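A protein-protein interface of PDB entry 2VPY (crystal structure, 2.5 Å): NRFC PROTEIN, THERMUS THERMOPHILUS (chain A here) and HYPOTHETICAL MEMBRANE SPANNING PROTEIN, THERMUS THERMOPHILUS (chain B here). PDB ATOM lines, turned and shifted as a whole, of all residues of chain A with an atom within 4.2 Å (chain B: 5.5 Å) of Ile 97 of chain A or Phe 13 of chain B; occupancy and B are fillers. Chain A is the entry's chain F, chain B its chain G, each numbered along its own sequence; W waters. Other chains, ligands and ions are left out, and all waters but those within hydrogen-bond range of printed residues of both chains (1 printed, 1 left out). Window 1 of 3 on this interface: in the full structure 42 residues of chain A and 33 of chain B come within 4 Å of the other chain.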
ATOM      1  N   GLY A  94      21.475 -24.104  17.915  1.00  0.00           N
ATOM      2  CA  GLY A  94      20.956 -22.746  17.891  1.00  0.00           C
ATOM      3  C   GLY A  94      20.844 -22.037  16.541  1.00  0.00           C
ATOM      4  O   GLY A  94      20.451 -20.868  16.498  1.00  0.00           O
ATOM      5  N   ALA A  95      21.128 -22.705  15.428  1.00  0.00           N
ATOM      6  CA  ALA A  95      21.069 -21.996  14.149  1.00  0.00           C
ATOM      7  C   ALA A  95      19.705 -21.391  13.854  1.00  0.00           C
ATOM      8  O   ALA A  95      19.609 -20.307  13.268  1.00  0.00           O
ATOM      9  CB  ALA A  95      21.513 -22.903  12.979  1.00  0.00           C
ATOM     10  N   CYS A  96      18.665 -22.100  14.283  1.00  0.00           N
ATOM     11  CA  CYS A  96      17.277 -21.707  14.100  1.00  0.00           C
ATOM     12  C   CYS A  96      16.933 -20.501  14.987  1.00  0.00           C
ATOM     13  O   CYS A  96      16.162 -19.629  14.577  1.00  0.00           O
ATOM     14  CB  CYS A  96      16.362 -22.903  14.393  1.00  0.00           C
ATOM     15  SG  CYS A  96      16.676 -23.719  16.035  1.00  0.00           S
ATOM     16  N   ILE A  97      17.489 -20.457  16.199  1.00  0.00           N
ATOM     17  CA  ILE A  97      17.264 -19.332  17.103  1.00  0.00           C
ATOM     18  C   ILE A  97      17.913 -18.101  16.441  1.00  0.00           C
ATOM     19  O   ILE A  97      17.319 -17.020  16.411  1.00  0.00           O
ATOM     20  CB  ILE A  97      17.865 -19.590  18.536  1.00  0.00           C
ATOM     21  CG1 ILE A  97      16.976 -20.586  19.290  1.00  0.00           C
ATOM     22  CG2 ILE A  97      17.965 -18.274  19.328  1.00  0.00           C
ATOM     23  CD1 ILE A  97      17.664 -21.333  20.413  1.00  0.00           C
ATOM     24  N   ALA A  98      19.115 -18.262  15.890  1.00  0.00           N
ATOM     25  CA  ALA A  98      19.782 -17.164  15.184  1.00  0.00           C
ATOM     26  C   ALA A  98      18.957 -16.670  13.963  1.00  0.00           C
ATOM     27  O   ALA A  98      18.890 -15.471  13.700  1.00  0.00           O
ATOM     28  CB  ALA A  98      21.183 -17.610  14.718  1.00  0.00           C
ATOM     29  N   ALA A  99      18.324 -17.592  13.244  1.00  0.00           N
ATOM     30  CA  ALA A  99      17.538 -17.232  12.071  1.00  0.00           C
ATOM     31  C   ALA A  99      16.071 -16.821  12.349  1.00  0.00           C
ATOM     32  O   ALA A  99      15.404 -16.291  11.462  1.00  0.00           O
ATOM     33  CB  ALA A  99      17.597 -18.390  11.030  1.00  0.00           C
ATOM     34  N   CYS A 100      15.569 -17.076  13.558  1.00  0.00           N
ATOM     35  CA  CYS A 100      14.197 -16.686  13.909  1.00  0.00           C
ATOM     36  C   CYS A 100      14.230 -15.164  14.194  1.00  0.00           C
ATOM     37  O   CYS A 100      15.027 -14.706  15.022  1.00  0.00           O
ATOM     38  CB  CYS A 100      13.654 -17.440  15.150  1.00  0.00           C
ATOM     39  SG  CYS A 100      11.929 -16.908  15.571  1.00  0.00           S
ATOM     40  N   ARG A 105      11.791 -18.936  19.775  1.00  0.00           N
ATOM     41  CA  ARG A 105      12.531 -20.165  20.054  1.00  0.00           C
ATOM     42  C   ARG A 105      13.425 -20.219  21.281  1.00  0.00           C
ATOM     43  O   ARG A 105      14.136 -19.261  21.566  1.00  0.00           O
ATOM     44  CB  ARG A 105      13.455 -20.483  18.869  1.00  0.00           C
ATOM     45  CG  ARG A 105      12.806 -20.618  17.527  1.00  0.00           C
ATOM     46  CD  ARG A 105      13.635 -21.492  16.609  1.00  0.00           C
ATOM     47  NE  ARG A 105      12.736 -22.099  15.647  1.00  0.00           N
ATOM     48  CZ  ARG A 105      12.714 -23.383  15.329  1.00  0.00           C
ATOM     49  NH1 ARG A 105      13.567 -24.228  15.891  1.00  0.00           N
ATOM     50  NH2 ARG A 105      11.797 -23.815  14.473  1.00  0.00           N
ATOM     51  N   VAL A 113      15.765 -27.705  21.118  1.00  0.00           N
ATOM     52  CA  VAL A 113      15.096 -26.442  20.894  1.00  0.00           C
ATOM     53  C   VAL A 113      13.579 -26.620  20.874  1.00  0.00           C
ATOM     54  O   VAL A 113      13.054 -27.618  20.368  1.00  0.00           O
ATOM     55  CB  VAL A 113      15.725 -25.778  19.602  1.00  0.00           C
ATOM     56  CG1 VAL A 113      14.875 -24.649  19.064  1.00  0.00           C
ATOM     57  CG2 VAL A 113      17.131 -25.235  19.966  1.00  0.00           C
ATOM     58  N   ASN B   9      12.141 -14.700  24.164  1.00  0.00           N
ATOM     59  CA  ASN B   9      13.360 -15.485  24.304  1.00  0.00           C
ATOM     60  C   ASN B   9      14.486 -14.761  23.533  1.00  0.00           C
ATOM     61  O   ASN B   9      14.983 -15.258  22.525  1.00  0.00           O
ATOM     62  CB  ASN B   9      13.116 -16.897  23.758  1.00  0.00           C
ATOM     63  CG  ASN B   9      11.933 -17.603  24.442  1.00  0.00           C
ATOM     64  OD1 ASN B   9      10.856 -17.777  23.849  1.00  0.00           O
ATOM     65  ND2 ASN B   9      12.136 -18.006  25.695  1.00  0.00           N
ATOM     66  N   GLN B  11      17.425 -13.920  24.830  1.00  0.00           N
ATOM     67  CA  GLN B  11      18.625 -14.223  25.595  1.00  0.00           C
ATOM     68  C   GLN B  11      19.775 -14.697  24.658  1.00  0.00           C
ATOM     69  O   GLN B  11      19.522 -15.317  23.625  1.00  0.00           O
ATOM     70  CB  GLN B  11      18.266 -15.338  26.624  1.00  0.00           C
ATOM     71  CG  GLN B  11      16.699 -15.562  26.881  1.00  0.00           C
ATOM     72  CD  GLN B  11      16.046 -16.814  26.192  1.00  0.00           C
ATOM     73  OE1 GLN B  11      16.432 -17.208  25.087  1.00  0.00           O
ATOM     74  NE2 GLN B  11      15.037 -17.409  26.852  1.00  0.00           N
ATOM     75  N   GLU B  12      21.022 -14.375  24.990  1.00  0.00           N
ATOM     76  CA  GLU B  12      22.187 -14.841  24.222  1.00  0.00           C
ATOM     77  C   GLU B  12      22.028 -16.373  23.917  1.00  0.00           C
ATOM     78  O   GLU B  12      21.644 -17.133  24.813  1.00  0.00           O
ATOM     79  CB  GLU B  12      23.441 -14.608  25.073  1.00  0.00           C
ATOM     80  CG  GLU B  12      24.728 -15.051  24.437  1.00  0.00           C
ATOM     81  CD  GLU B  12      25.943 -14.821  25.323  1.00  0.00           C
ATOM     82  OE1 GLU B  12      26.156 -15.615  26.272  1.00  0.00           O
ATOM     83  OE2 GLU B  12      26.678 -13.836  25.071  1.00  0.00           O
ATOM     84  N   PHE B  13      22.309 -16.834  22.691  1.00  0.00           N
ATOM     85  CA  PHE B  13      22.163 -18.261  22.359  1.00  0.00           C
ATOM     86  C   PHE B  13      23.503 -18.987  22.100  1.00  0.00           C
ATOM     87  O   PHE B  13      23.599 -20.214  22.236  1.00  0.00           O
ATOM     88  CB  PHE B  13      21.177 -18.439  21.172  1.00  0.00           C
ATOM     89  CG  PHE B  13      21.426 -17.504  20.016  1.00  0.00           C
ATOM     90  CD1 PHE B  13      22.418 -17.788  19.080  1.00  0.00           C
ATOM     91  CD2 PHE B  13      20.708 -16.304  19.899  1.00  0.00           C
ATOM     92  CE1 PHE B  13      22.700 -16.896  18.042  1.00  0.00           C
ATOM     93  CE2 PHE B  13      20.980 -15.402  18.867  1.00  0.00           C
ATOM     94  CZ  PHE B  13      21.979 -15.697  17.936  1.00  0.00           C
ATOM     95  N   TRP B  14      24.534 -18.222  21.740  1.00  0.00           N
ATOM     96  CA  TRP B  14      25.890 -18.750  21.490  1.00  0.00           C
ATOM     97  C   TRP B  14      26.770 -17.996  22.471  1.00  0.00           C
ATOM     98  O   TRP B  14      27.022 -16.804  22.333  1.00  0.00           O
ATOM     99  CB  TRP B  14      26.363 -18.523  20.037  1.00  0.00           C
ATOM    100  CG  TRP B  14      25.676 -19.410  18.980  1.00  0.00           C
ATOM    101  CD1 TRP B  14      25.083 -20.637  19.172  1.00  0.00           C
ATOM    102  CD2 TRP B  14      25.501 -19.100  17.587  1.00  0.00           C
ATOM    103  NE1 TRP B  14      24.550 -21.095  17.985  1.00  0.00           N
ATOM    104  CE2 TRP B  14      24.794 -20.174  16.999  1.00  0.00           C
ATOM    105  CE3 TRP B  14      25.879 -18.017  16.782  1.00  0.00           C
ATOM    106  CZ2 TRP B  14      24.442 -20.190  15.638  1.00  0.00           C
ATOM    107  CZ3 TRP B  14      25.534 -18.026  15.430  1.00  0.00           C
ATOM    108  CH2 TRP B  14      24.823 -19.111  14.873  1.00  0.00           C
ATOM    109  N   HIS B  15      27.234 -18.721  23.470  1.00  0.00           N
ATOM    110  CA  HIS B  15      28.006 -18.152  24.558  1.00  0.00           C
ATOM    111  C   HIS B  15      29.499 -18.120  24.335  1.00  0.00           C
ATOM    112  O   HIS B  15      29.979 -18.556  23.292  1.00  0.00           O
ATOM    113  CB  HIS B  15      27.682 -18.955  25.821  1.00  0.00           C
ATOM    114  CG  HIS B  15      26.225 -19.231  26.004  1.00  0.00           C
ATOM    115  ND1 HIS B  15      25.343 -18.272  26.434  1.00  0.00           N
ATOM    116  CD2 HIS B  15      25.493 -20.343  25.786  1.00  0.00           C
ATOM    117  CE1 HIS B  15      24.128 -18.782  26.475  1.00  0.00           C
ATOM    118  NE2 HIS B  15      24.192 -20.039  26.085  1.00  0.00           N
ATOM    119  N   ASN B 140      17.998 -11.291   9.829  1.00  0.00           N
ATOM    120  CA  ASN B 140      17.281 -10.582  10.904  1.00  0.00           C
ATOM    121  C   ASN B 140      18.226  -9.939  11.941  1.00  0.00           C
ATOM    122  O   ASN B 140      17.795  -9.193  12.813  1.00  0.00           O
ATOM    123  CB  ASN B 140      16.316 -11.520  11.666  1.00  0.00           C
ATOM    124  CG  ASN B 140      16.963 -12.851  12.077  1.00  0.00           C
ATOM    125  OD1 ASN B 140      16.904 -13.270  13.251  1.00  0.00           O
ATOM    126  ND2 ASN B 140      17.566 -13.532  11.103  1.00  0.00           N
ATOM    127  N   ARG B 141      19.512 -10.241  11.840  1.00  0.00           N
ATOM    128  CA  ARG B 141      20.534  -9.745  12.768  1.00  0.00           C
ATOM    129  C   ARG B 141      21.289  -8.614  12.072  1.00  0.00           C
ATOM    130  O   ARG B 141      22.224  -8.855  11.329  1.00  0.00           O
ATOM    131  CB  ARG B 141      21.450 -10.920  13.103  1.00  0.00           C
ATOM    132  CG  ARG B 141      20.676 -12.181  13.530  1.00  0.00           C
ATOM    133  CD  ARG B 141      20.314 -12.099  14.993  1.00  0.00           C
ATOM    134  NE  ARG B 141      19.422 -13.149  15.468  1.00  0.00           N
ATOM    135  CZ  ARG B 141      18.966 -13.178  16.712  1.00  0.00           C
ATOM    136  NH1 ARG B 141      19.343 -12.219  17.535  1.00  0.00           N
ATOM    137  NH2 ARG B 141      18.143 -14.127  17.130  1.00  0.00           N
ATOM    138  N   TRP B 144      25.287  -8.859  11.760  1.00  0.00           N
ATOM    139  CA  TRP B 144      25.858  -9.913  10.948  1.00  0.00           C
ATOM    140  C   TRP B 144      25.590  -9.697   9.457  1.00  0.00           C
ATOM    141  O   TRP B 144      24.946 -10.522   8.823  1.00  0.00           O
ATOM    142  CB  TRP B 144      25.341 -11.284  11.401  1.00  0.00           C
ATOM    143  CG  TRP B 144      25.870 -11.685  12.767  1.00  0.00           C
ATOM    144  CD1 TRP B 144      26.934 -11.130  13.429  1.00  0.00           C
ATOM    145  CD2 TRP B 144      25.349 -12.706  13.636  1.00  0.00           C
ATOM    146  NE1 TRP B 144      27.105 -11.739  14.649  1.00  0.00           N
ATOM    147  CE2 TRP B 144      26.149 -12.707  14.804  1.00  0.00           C
ATOM    148  CE3 TRP B 144      24.287 -13.615  13.542  1.00  0.00           C
ATOM    149  CZ2 TRP B 144      25.917 -13.587  15.877  1.00  0.00           C
ATOM    150  CZ3 TRP B 144      24.052 -14.494  14.606  1.00  0.00           C
ATOM    151  CH2 TRP B 144      24.872 -14.469  15.760  1.00  0.00           C
ATOM    152  N   GLN B 247      24.281 -10.928  18.342  1.00  0.00           N
ATOM    153  CA  GLN B 247      23.077 -11.682  18.699  1.00  0.00           C
ATOM    154  C   GLN B 247      21.992 -10.720  19.121  1.00  0.00           C
ATOM    155  O   GLN B 247      21.359 -10.867  20.161  1.00  0.00           O
ATOM    156  CB  GLN B 247      23.404 -12.629  19.828  1.00  0.00           C
ATOM    157  CG  GLN B 247      24.181 -13.799  19.339  1.00  0.00           C
ATOM    158  CD  GLN B 247      24.796 -14.600  20.450  1.00  0.00           C
ATOM    159  OE1 GLN B 247      24.107 -15.320  21.171  1.00  0.00           O
ATOM    160  NE2 GLN B 247      26.108 -14.472  20.603  1.00  0.00           N
ATOM    161  N   GLN B 249      18.701  -8.341  17.534  1.00  0.00           N
ATOM    162  CA  GLN B 249      17.627  -8.510  16.574  1.00  0.00           C
ATOM    163  C   GLN B 249      17.154  -7.182  16.110  1.00  0.00           C
ATOM    164  O   GLN B 249      16.582  -6.984  15.029  1.00  0.00           O
ATOM    165  CB  GLN B 249      16.545  -9.101  17.487  1.00  0.00           C
ATOM    166  CG  GLN B 249      15.334  -9.774  16.970  1.00  0.00           C
ATOM    167  CD  GLN B 249      15.657 -11.103  16.354  1.00  0.00           C
ATOM    168  OE1 GLN B 249      15.440 -12.172  16.941  1.00  0.00           O
ATOM    169  NE2 GLN B 249      16.194 -11.047  15.152  1.00  0.00           N
HETATM  170  O   HOH W   1      16.508 -15.040   9.468  1.00  0.00           O
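The guanidinium group of Arg 141 of chain B lies within hydrogen-bond range of the backbone carbonyl oxygen of Ile 97 of chain A (3.1 Å).
The backbone carbonyl oxygen (O) of Ala 98 of chain A lies close to the side-chain amide oxygen (OD1) of Asn 140 of chain B, at 3.0 Å.
The backbone carbonyl oxygen (O) of Ala 98 of chain A sits at hydrogen-bond distance from the guanidinium group (NE) of Arg 141 of chain B, at 3.0 Å.
The backbone carbonyl oxygen (O) of Cys 100 of chain A lies close to the side-chain amide oxygen (OD1) of Asn 140 of chain B, at 3.0 Å.
O of Cys 100 of chain A sits close to OE1 of Gln 249 of chain B (3.2 Å).
Gly 94 of chain A touches Trp 14 of chain B.
Phe 13 of chain B touches Ile 97 of chain A.
Phe 13 of chain B touches Ala 98 of chain A.
Trp 14 of chain B touches Ala 98 of chain A.
Ala 99 of chain A touches Asn 140 of chain B (O to ND2, 3.5 Å).
O of Cys 100 of chain A touches NH2 of Arg 141 of chain B, 3.8 Å away.
Asn 9 of chain B touches Arg 105 of chain A (CB to O, 3.4 Å).
SG of Cys 96 of chain A sits close to NH1 of Arg 105 of chain A (3.2 Å).
The side-chain amide nitrogen (ND2) of Asn 9 of chain B lies close to the side-chain amide nitrogen (NE2) of Gln 11 of chain B (3.2 Å).
N of Trp 14 of chain B is in hydrogen-bond range of OE1 of Gln 247 of chain B (3.0 Å).
The guanidinium group of Arg 141 of chain B lies within hydrogen-bond range of the side-chain amide oxygen of Asn 140 of chain B.
OD1 of Asn 140 of chain B lies within hydrogen-bond range of NE2 of Gln 249 of chain B, 3.0 Å away.
OE1 of Gln 249 of chain B sits at hydrogen-bond distance from NH2 of Arg 141 of chain B.
Water W1 lies within hydrogen-bond range of ND2 of Asn 140 of chain B (2.5 Å) and O of Ala 99 of chain A (2.6 Å).
Along chain A the printed residues that touch a printed residue of chain B span positions 94 to 105.
Of the 11 printed residues of chain B, 6 touch a printed residue of chain A.
Printed residues of chain B that touch a printed residue of chain A: Asn 9, Phe 13, Trp 14, Asn 140, Arg 141 and Gln 249.
Among the printed residues, no Asp or Glu carboxylate lies within 4 Å of a Lys or Arg side-chain nitrogen of the other chain.
Ile 97 of chain A touches two residues of chain B.
Phe 13 of chain B touches two residues of chain A.
Of the printed residues of chain B, Cys 100 of chain A touches Asn 140, Arg 141 and Gln 249.
Printed residues of chain B within 4 Å of Arg 105 of chain A: Asn 9 (3.4 Å).
Of the printed residues of chain A, Trp 14 of chain B touches Gly 94 and Ala 98.
Gln 11 of chain B touches none of the printed residues of chain A.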
